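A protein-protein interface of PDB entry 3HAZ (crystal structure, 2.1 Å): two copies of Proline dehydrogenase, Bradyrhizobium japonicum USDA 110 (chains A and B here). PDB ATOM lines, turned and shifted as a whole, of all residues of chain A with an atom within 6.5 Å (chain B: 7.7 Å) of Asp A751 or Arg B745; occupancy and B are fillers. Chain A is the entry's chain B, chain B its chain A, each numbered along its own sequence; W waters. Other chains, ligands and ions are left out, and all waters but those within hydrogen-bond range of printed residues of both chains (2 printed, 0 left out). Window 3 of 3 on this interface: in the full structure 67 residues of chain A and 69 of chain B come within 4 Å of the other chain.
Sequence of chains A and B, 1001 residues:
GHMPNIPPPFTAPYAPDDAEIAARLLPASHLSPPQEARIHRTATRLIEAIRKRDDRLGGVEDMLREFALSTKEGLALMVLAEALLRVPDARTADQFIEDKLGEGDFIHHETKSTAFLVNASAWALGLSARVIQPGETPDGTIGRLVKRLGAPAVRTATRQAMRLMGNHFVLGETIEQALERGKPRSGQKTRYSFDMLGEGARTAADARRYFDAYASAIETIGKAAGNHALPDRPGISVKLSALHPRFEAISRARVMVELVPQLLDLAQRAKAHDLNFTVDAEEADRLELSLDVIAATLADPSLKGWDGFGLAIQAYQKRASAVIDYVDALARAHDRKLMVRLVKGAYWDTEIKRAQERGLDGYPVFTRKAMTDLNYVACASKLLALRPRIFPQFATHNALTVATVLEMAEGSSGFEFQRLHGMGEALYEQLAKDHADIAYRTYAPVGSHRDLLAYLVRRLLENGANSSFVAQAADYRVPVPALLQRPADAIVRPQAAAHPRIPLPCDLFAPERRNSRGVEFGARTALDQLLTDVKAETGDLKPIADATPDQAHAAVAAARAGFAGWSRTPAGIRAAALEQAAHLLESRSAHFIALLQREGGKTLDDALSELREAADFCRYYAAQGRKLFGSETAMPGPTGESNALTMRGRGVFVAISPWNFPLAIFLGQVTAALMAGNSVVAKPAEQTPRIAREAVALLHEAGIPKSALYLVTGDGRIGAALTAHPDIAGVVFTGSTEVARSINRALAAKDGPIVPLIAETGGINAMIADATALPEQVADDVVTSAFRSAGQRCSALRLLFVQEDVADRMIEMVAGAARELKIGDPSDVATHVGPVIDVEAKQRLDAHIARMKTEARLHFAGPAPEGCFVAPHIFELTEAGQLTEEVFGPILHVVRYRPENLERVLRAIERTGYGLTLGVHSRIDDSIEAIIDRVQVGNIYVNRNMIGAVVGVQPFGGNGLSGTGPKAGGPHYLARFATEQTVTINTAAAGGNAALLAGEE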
ATOM      1  N   ARG A 745      18.102 -20.752 -14.831  1.00  0.00           N
ATOM      2  CA  ARG A 745      17.654 -21.880 -14.017  1.00  0.00           C
ATOM      3  C   ARG A 745      18.664 -22.239 -12.937  1.00  0.00           C
ATOM      4  O   ARG A 745      18.288 -22.578 -11.816  1.00  0.00           O
ATOM      5  CB  ARG A 745      17.352 -23.094 -14.893  1.00  0.00           C
ATOM      6  CG  ARG A 745      15.984 -23.005 -15.543  1.00  0.00           C
ATOM      7  CD  ARG A 745      15.886 -23.813 -16.814  1.00  0.00           C
ATOM      8  NE  ARG A 745      14.741 -23.362 -17.595  1.00  0.00           N
ATOM      9  CZ  ARG A 745      14.536 -23.655 -18.874  1.00  0.00           C
ATOM     10  NH1 ARG A 745      13.459 -23.189 -19.492  1.00  0.00           N
ATOM     11  NH2 ARG A 745      15.406 -24.412 -19.533  1.00  0.00           N
ATOM     12  N   LEU A 747      20.750 -20.117 -11.558  1.00  0.00           N
ATOM     13  CA  LEU A 747      20.622 -19.078 -10.542  1.00  0.00           C
ATOM     14  C   LEU A 747      19.413 -19.344  -9.645  1.00  0.00           C
ATOM     15  O   LEU A 747      19.524 -19.334  -8.420  1.00  0.00           O
ATOM     16  CB  LEU A 747      20.541 -17.685 -11.183  1.00  0.00           C
ATOM     17  CG  LEU A 747      21.811 -17.266 -11.934  1.00  0.00           C
ATOM     18  CD1 LEU A 747      21.615 -15.945 -12.668  1.00  0.00           C
ATOM     19  CD2 LEU A 747      22.997 -17.186 -10.980  1.00  0.00           C
ATOM     20  N   ALA A 748      18.263 -19.605 -10.259  1.00  0.00           N
ATOM     21  CA  ALA A 748      17.027 -19.805  -9.508  1.00  0.00           C
ATOM     22  C   ALA A 748      17.115 -20.985  -8.542  1.00  0.00           C
ATOM     23  O   ALA A 748      16.484 -20.982  -7.482  1.00  0.00           O
ATOM     24  CB  ALA A 748      15.851 -19.989 -10.461  1.00  0.00           C
ATOM     25  N   ALA A 749      17.892 -21.996  -8.919  1.00  0.00           N
ATOM     26  CA  ALA A 749      18.008 -23.215  -8.126  1.00  0.00           C
ATOM     27  C   ALA A 749      18.682 -23.002  -6.770  1.00  0.00           C
ATOM     28  O   ALA A 749      18.407 -23.733  -5.821  1.00  0.00           O
ATOM     29  CB  ALA A 749      18.742 -24.300  -8.924  1.00  0.00           C
ATOM     30  N   LYS A 750      19.560 -22.006  -6.675  1.00  0.00           N
ATOM     31  CA  LYS A 750      20.300 -21.763  -5.433  1.00  0.00           C
ATOM     32  C   LYS A 750      19.378 -21.343  -4.298  1.00  0.00           C
ATOM     33  O   LYS A 750      18.328 -20.729  -4.526  1.00  0.00           O
ATOM     34  CB  LYS A 750      21.359 -20.681  -5.630  1.00  0.00           C
ATOM     35  CG  LYS A 750      22.290 -20.888  -6.811  1.00  0.00           C
ATOM     36  CD  LYS A 750      23.195 -19.675  -6.972  1.00  0.00           C
ATOM     37  CE  LYS A 750      24.148 -19.823  -8.141  1.00  0.00           C
ATOM     38  NZ  LYS A 750      25.044 -18.640  -8.256  1.00  0.00           N
ATOM     39  N   ASP A 751      19.788 -21.646  -3.069  1.00  0.00           N
ATOM     40  CA  ASP A 751      19.015 -21.258  -1.900  1.00  0.00           C
ATOM     41  C   ASP A 751      19.363 -19.847  -1.439  1.00  0.00           C
ATOM     42  O   ASP A 751      18.665 -19.267  -0.610  1.00  0.00           O
ATOM     43  CB  ASP A 751      19.222 -22.267  -0.769  1.00  0.00           C
ATOM     44  CG  ASP A 751      18.612 -23.618  -1.086  1.00  0.00           C
ATOM     45  OD1 ASP A 751      17.486 -23.648  -1.630  1.00  0.00           O
ATOM     46  OD2 ASP A 751      19.257 -24.646  -0.795  1.00  0.00           O
ATOM     47  N   GLY A 752      20.437 -19.290  -1.993  1.00  0.00           N
ATOM     48  CA  GLY A 752      20.896 -17.972  -1.592  1.00  0.00           C
ATOM     49  C   GLY A 752      20.059 -16.822  -2.139  1.00  0.00           C
ATOM     50  O   GLY A 752      18.893 -16.996  -2.493  1.00  0.00           O
ATOM     51  N   PRO A 753      20.651 -15.625  -2.195  1.00  0.00           N
ATOM     52  CA  PRO A 753      19.955 -14.446  -2.725  1.00  0.00           C
ATOM     53  C   PRO A 753      19.583 -14.590  -4.196  1.00  0.00           C
ATOM     54  O   PRO A 753      20.347 -15.165  -4.981  1.00  0.00           O
ATOM     55  CB  PRO A 753      20.990 -13.332  -2.561  1.00  0.00           C
ATOM     56  CG  PRO A 753      21.848 -13.789  -1.405  1.00  0.00           C
ATOM     57  CD  PRO A 753      21.941 -15.280  -1.567  1.00  0.00           C
ATOM     58  N   THR B 737      10.966 -15.002   2.094  1.00  0.00           N
ATOM     59  CA  THR B 737      12.129 -15.318   1.276  1.00  0.00           C
ATOM     60  C   THR B 737      11.951 -16.665   0.584  1.00  0.00           C
ATOM     61  O   THR B 737      12.364 -16.849  -0.563  1.00  0.00           O
ATOM     62  CB  THR B 737      13.419 -15.345   2.118  1.00  0.00           C
ATOM     63  OG1 THR B 737      13.570 -14.096   2.804  1.00  0.00           O
ATOM     64  CG2 THR B 737      14.630 -15.575   1.231  1.00  0.00           C
ATOM     65  N   GLU B 738      11.314 -17.598   1.280  1.00  0.00           N
ATOM     66  CA  GLU B 738      11.135 -18.949   0.762  1.00  0.00           C
ATOM     67  C   GLU B 738      10.173 -18.990  -0.422  1.00  0.00           C
ATOM     68  O   GLU B 738      10.415 -19.681  -1.421  1.00  0.00           O
ATOM     69  CB  GLU B 738      10.646 -19.885   1.873  1.00  0.00           C
ATOM     70  N   VAL B 739       9.071 -18.261  -0.309  1.00  0.00           N
ATOM     71  CA  VAL B 739       8.099 -18.214  -1.392  1.00  0.00           C
ATOM     72  C   VAL B 739       8.683 -17.511  -2.629  1.00  0.00           C
ATOM     73  O   VAL B 739       8.413 -17.908  -3.760  1.00  0.00           O
ATOM     74  CB  VAL B 739       6.777 -17.560  -0.940  1.00  0.00           C
ATOM     75  CG1 VAL B 739       5.892 -17.247  -2.143  1.00  0.00           C
ATOM     76  CG2 VAL B 739       6.047 -18.474   0.044  1.00  0.00           C
ATOM     77  N   ALA B 740       9.507 -16.490  -2.411  1.00  0.00           N
ATOM     78  CA  ALA B 740      10.126 -15.779  -3.524  1.00  0.00           C
ATOM     79  C   ALA B 740      10.978 -16.718  -4.377  1.00  0.00           C
ATOM     80  O   ALA B 740      10.895 -16.698  -5.605  1.00  0.00           O
ATOM     81  CB  ALA B 740      10.950 -14.586  -3.026  1.00  0.00           C
ATOM     82  N   ARG B 741      11.784 -17.551  -3.725  1.00  0.00           N
ATOM     83  CA  ARG B 741      12.623 -18.514  -4.436  1.00  0.00           C
ATOM     84  C   ARG B 741      11.785 -19.496  -5.243  1.00  0.00           C
ATOM     85  O   ARG B 741      12.161 -19.893  -6.347  1.00  0.00           O
ATOM     86  CB  ARG B 741      13.519 -19.282  -3.460  1.00  0.00           C
ATOM     87  CG  ARG B 741      14.700 -18.481  -2.944  1.00  0.00           C
ATOM     88  CD  ARG B 741      15.785 -19.407  -2.439  1.00  0.00           C
ATOM     89  NE  ARG B 741      15.365 -20.119  -1.237  1.00  0.00           N
ATOM     90  CZ  ARG B 741      15.463 -19.618  -0.011  1.00  0.00           C
ATOM     91  NH1 ARG B 741      15.967 -18.403   0.169  1.00  0.00           N
ATOM     92  NH2 ARG B 741      15.055 -20.325   1.030  1.00  0.00           N
ATOM     93  N   SER B 742      10.650 -19.895  -4.680  1.00  0.00           N
ATOM     94  CA  SER B 742       9.732 -20.792  -5.364  1.00  0.00           C
ATOM     95  C   SER B 742       9.174 -20.128  -6.624  1.00  0.00           C
ATOM     96  O   SER B 742       9.111 -20.744  -7.691  1.00  0.00           O
ATOM     97  CB  SER B 742       8.598 -21.205  -4.421  1.00  0.00           C
ATOM     98  OG  SER B 742       7.506 -21.746  -5.149  1.00  0.00           O
ATOM     99  N   ILE B 743       8.774 -18.866  -6.493  1.00  0.00           N
ATOM    100  CA  ILE B 743       8.295 -18.093  -7.636  1.00  0.00           C
ATOM    101  C   ILE B 743       9.392 -17.951  -8.682  1.00  0.00           C
ATOM    102  O   ILE B 743       9.162 -18.169  -9.871  1.00  0.00           O
ATOM    103  CB  ILE B 743       7.815 -16.691  -7.214  1.00  0.00           C
ATOM    104  CG1 ILE B 743       6.430 -16.779  -6.566  1.00  0.00           C
ATOM    105  CG2 ILE B 743       7.785 -15.755  -8.418  1.00  0.00           C
ATOM    106  CD1 ILE B 743       6.056 -15.549  -5.753  1.00  0.00           C
ATOM    107  N   ASN B 744      10.590 -17.597  -8.229  1.00  0.00           N
ATOM    108  CA  ASN B 744      11.724 -17.432  -9.126  1.00  0.00           C
ATOM    109  C   ASN B 744      12.002 -18.705  -9.923  1.00  0.00           C
ATOM    110  O   ASN B 744      12.273 -18.646 -11.122  1.00  0.00           O
ATOM    111  CB  ASN B 744      12.968 -17.004  -8.342  1.00  0.00           C
ATOM    112  CG  ASN B 744      14.047 -16.430  -9.237  1.00  0.00           C
ATOM    113  OD1 ASN B 744      13.754 -15.826 -10.269  1.00  0.00           O
ATOM    114  ND2 ASN B 744      15.303 -16.616  -8.846  1.00  0.00           N
ATOM    115  N   ARG B 745      11.922 -19.855  -9.256  1.00  0.00           N
ATOM    116  CA  ARG B 745      12.138 -21.132  -9.926  1.00  0.00           C
ATOM    117  C   ARG B 745      11.058 -21.414 -10.963  1.00  0.00           C
ATOM    118  O   ARG B 745      11.364 -21.854 -12.065  1.00  0.00           O
ATOM    119  CB  ARG B 745      12.234 -22.277  -8.917  1.00  0.00           C
ATOM    120  CG  ARG B 745      13.603 -22.373  -8.252  1.00  0.00           C
ATOM    121  CD  ARG B 745      13.551 -23.034  -6.883  1.00  0.00           C
ATOM    122  NE  ARG B 745      14.754 -22.714  -6.114  1.00  0.00           N
ATOM    123  CZ  ARG B 745      14.917 -22.981  -4.822  1.00  0.00           C
ATOM    124  NH1 ARG B 745      16.050 -22.645  -4.212  1.00  0.00           N
ATOM    125  NH2 ARG B 745      13.948 -23.580  -4.140  1.00  0.00           N
ATOM    126  N   ALA B 746       9.802 -21.155 -10.612  1.00  0.00           N
ATOM    127  CA  ALA B 746       8.704 -21.345 -11.553  1.00  0.00           C
ATOM    128  C   ALA B 746       8.879 -20.458 -12.788  1.00  0.00           C
ATOM    129  O   ALA B 746       8.612 -20.885 -13.908  1.00  0.00           O
ATOM    130  CB  ALA B 746       7.359 -21.087 -10.881  1.00  0.00           C
ATOM    131  N   LEU B 747       9.342 -19.226 -12.588  1.00  0.00           N
ATOM    132  CA  LEU B 747       9.604 -18.340 -13.718  1.00  0.00           C
ATOM    133  C   LEU B 747      10.750 -18.874 -14.581  1.00  0.00           C
ATOM    134  O   LEU B 747      10.632 -18.965 -15.800  1.00  0.00           O
ATOM    135  CB  LEU B 747       9.909 -16.915 -13.239  1.00  0.00           C
ATOM    136  CG  LEU B 747       8.735 -16.136 -12.639  1.00  0.00           C
ATOM    137  CD1 LEU B 747       9.194 -14.803 -12.058  1.00  0.00           C
ATOM    138  CD2 LEU B 747       7.660 -15.920 -13.687  1.00  0.00           C
ATOM    139  N   ALA B 748      11.857 -19.234 -13.944  1.00  0.00           N
ATOM    140  CA  ALA B 748      13.035 -19.687 -14.675  1.00  0.00           C
ATOM    141  C   ALA B 748      12.776 -20.981 -15.444  1.00  0.00           C
ATOM    142  O   ALA B 748      13.447 -21.263 -16.435  1.00  0.00           O
ATOM    143  CB  ALA B 748      14.213 -19.860 -13.732  1.00  0.00           C
ATOM    144  N   ALA B 749      11.811 -21.767 -14.974  1.00  0.00           N
ATOM    145  CA  ALA B 749      11.469 -23.033 -15.612  1.00  0.00           C
ATOM    146  C   ALA B 749      10.878 -22.842 -17.009  1.00  0.00           C
ATOM    147  O   ALA B 749      11.105 -23.655 -17.901  1.00  0.00           O
ATOM    148  CB  ALA B 749      10.502 -23.828 -14.726  1.00  0.00           C
ATOM    149  N   LYS B 750      10.123 -21.765 -17.200  1.00  0.00           N
ATOM    150  CA  LYS B 750       9.433 -21.541 -18.468  1.00  0.00           C
ATOM    151  C   LYS B 750      10.415 -21.449 -19.631  1.00  0.00           C
ATOM    152  O   LYS B 750      11.578 -21.090 -19.443  1.00  0.00           O
ATOM    153  CB  LYS B 750       8.599 -20.264 -18.395  1.00  0.00           C
ATOM    154  CG  LYS B 750       7.717 -20.171 -17.161  1.00  0.00           C
ATOM    155  CD  LYS B 750       7.153 -18.772 -17.004  1.00  0.00           C
ATOM    156  CE  LYS B 750       5.949 -18.755 -16.077  1.00  0.00           C
ATOM    157  NZ  LYS B 750       5.341 -17.392 -16.000  1.00  0.00           N
ATOM    158  N   LEU B 757      11.624 -10.249 -11.917  1.00  0.00           N
ATOM    159  CA  LEU B 757      11.036 -10.543 -10.619  1.00  0.00           C
ATOM    160  C   LEU B 757      11.510  -9.499  -9.618  1.00  0.00           C
ATOM    161  O   LEU B 757      12.705  -9.377  -9.351  1.00  0.00           O
ATOM    162  CB  LEU B 757      11.411 -11.950 -10.134  1.00  0.00           C
ATOM    163  CG  LEU B 757      11.075 -12.287  -8.673  1.00  0.00           C
ATOM    164  CD1 LEU B 757       9.594 -12.092  -8.389  1.00  0.00           C
ATOM    165  CD2 LEU B 757      11.487 -13.715  -8.314  1.00  0.00           C
ATOM    166  N   LEU B 961      19.425 -11.813   1.082  1.00  0.00           N
ATOM    167  CA  LEU B 961      18.200 -12.583   1.286  1.00  0.00           C
ATOM    168  C   LEU B 961      16.978 -11.699   1.556  1.00  0.00           C
ATOM    169  O   LEU B 961      15.858 -12.198   1.664  1.00  0.00           O
ATOM    170  CB  LEU B 961      18.378 -13.585   2.442  1.00  0.00           C
ATOM    171  CG  LEU B 961      19.497 -14.624   2.334  1.00  0.00           C
ATOM    172  CD1 LEU B 961      19.534 -15.546   3.577  1.00  0.00           C
ATOM    173  CD2 LEU B 961      19.351 -15.446   1.067  1.00  0.00           C
HETATM  174  O   HOH W   1      15.497 -18.529  -6.464  1.00  0.00           O
HETATM  175  O   HOH W   2      16.548 -15.884  -1.500  1.00  0.00           O
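Arg A745 touches Ala B748, and with the chains exchanged Ala A748 touches Arg B745. Arg A745 touches Ala B749, and with the chains exchanged Ala A749 touches Arg B745. Arg A745 touches Lys B750, and with the chains exchanged Lys A750 touches Arg B745. Ala B748 touches its own counterpart, Ala A748. 5 positions are printed for both chains. Of the 14 pairs that touch across the chains among the printed residues, 7 have their exchanged pair printed and touching as well.
Of the 8 printed residues of chain A, 7 touch a printed residue of chain B. Hydrophobic or aromatic side chains of chain A within 4 Å of the printed part of chain B: Ala A748 and Pro A753. Along chain A the printed residues that touch a printed residue of chain B span positions 745 to 753. Hydrophobic or aromatic side chains of chain B within 4 Å of the printed part of chain A: Ala B748 and Leu B961. Among the printed residues, 14 pairs touch across the chains.
Among the printed residues, merely in contact across the chains: Ala A748 with Asn B744 (3.7 Å), Ala A748 with Ala B748 (3.7 Å), Lys A750 with Arg B741 (3.5 Å), Gly A752 with Arg B741 (3.9 Å), Gly A752 with Leu B961 (3.6 Å) and Pro A753 with Leu B961 (3.5 Å).
Water W2 bridges O of Gly A752 (2.8 Å) and NH1 of Arg B741 (3.1 Å). Water W1 bridges O of Ala A748 (2.8 Å) and ND2 of Asn B744 (3.1 Å).
Asp A751 touches two residues of chain B. Of chain A, only Ala A748, Ala A749, Lys A750 and Asp A751 come within 4 Å of Arg B745. Of the printed residues of chain B, Lys A750 touches Arg B741 and Arg B745. Of the printed residues of chain A, Arg B741 touches Lys A750 (3.5 Å), Asp A751 (2.9 Å) and Gly A752 (3.9 Å). Of the printed residues of chain B, Pro A753 touches Leu B961 (3.5 Å). Printed residues of chain B within 4 Å of Ala A749: Arg B745 (3.1 Å). Ile B743 touches none of the printed residues of chain A. The nearest residue of chain B that does not touch Asp A751 is Leu B961 (4.2 Å). The nearest printed residue of chain B that does not touch Pro A753 is Arg B741 (5.9 Å).
The backbone carbonyl oxygen (O) of Leu B961 lies within hydrogen-bond range of the side-chain hydroxyl (OG1) of Thr B737, 3.2 Å away.
The backbone carbonyl oxygen (O) of Ala B749 sits at hydrogen-bond distance from the guanidinium group (NH1) of Arg A745 (2.9 Å). The guanidinium group of Arg B745 lies within salt-bridge range of the side-chain carboxylate of Asp A751 (3.1 Å). O of Lys B750 is in hydrogen-bond range of NH1 of Arg A745 (2.8 Å). O of Asp A751 lies within hydrogen-bond range of NH1 of Arg B741, at 2.9 Å. The backbone carbonyl oxygen (O) of Ala B748 lies within hydrogen-bond range of the guanidinium group (NE) of Arg A745 (2.7 Å). NH1 of Arg B745 lies within hydrogen-bond range of O of Lys A750 (3.0 Å). O of Ala A748 is in hydrogen-bond range of NE of Arg B745. The backbone carbonyl oxygen (O) of Ala A749 lies within hydrogen-bond range of the guanidinium group (NH1) of Arg B745, 3.1 Å away.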
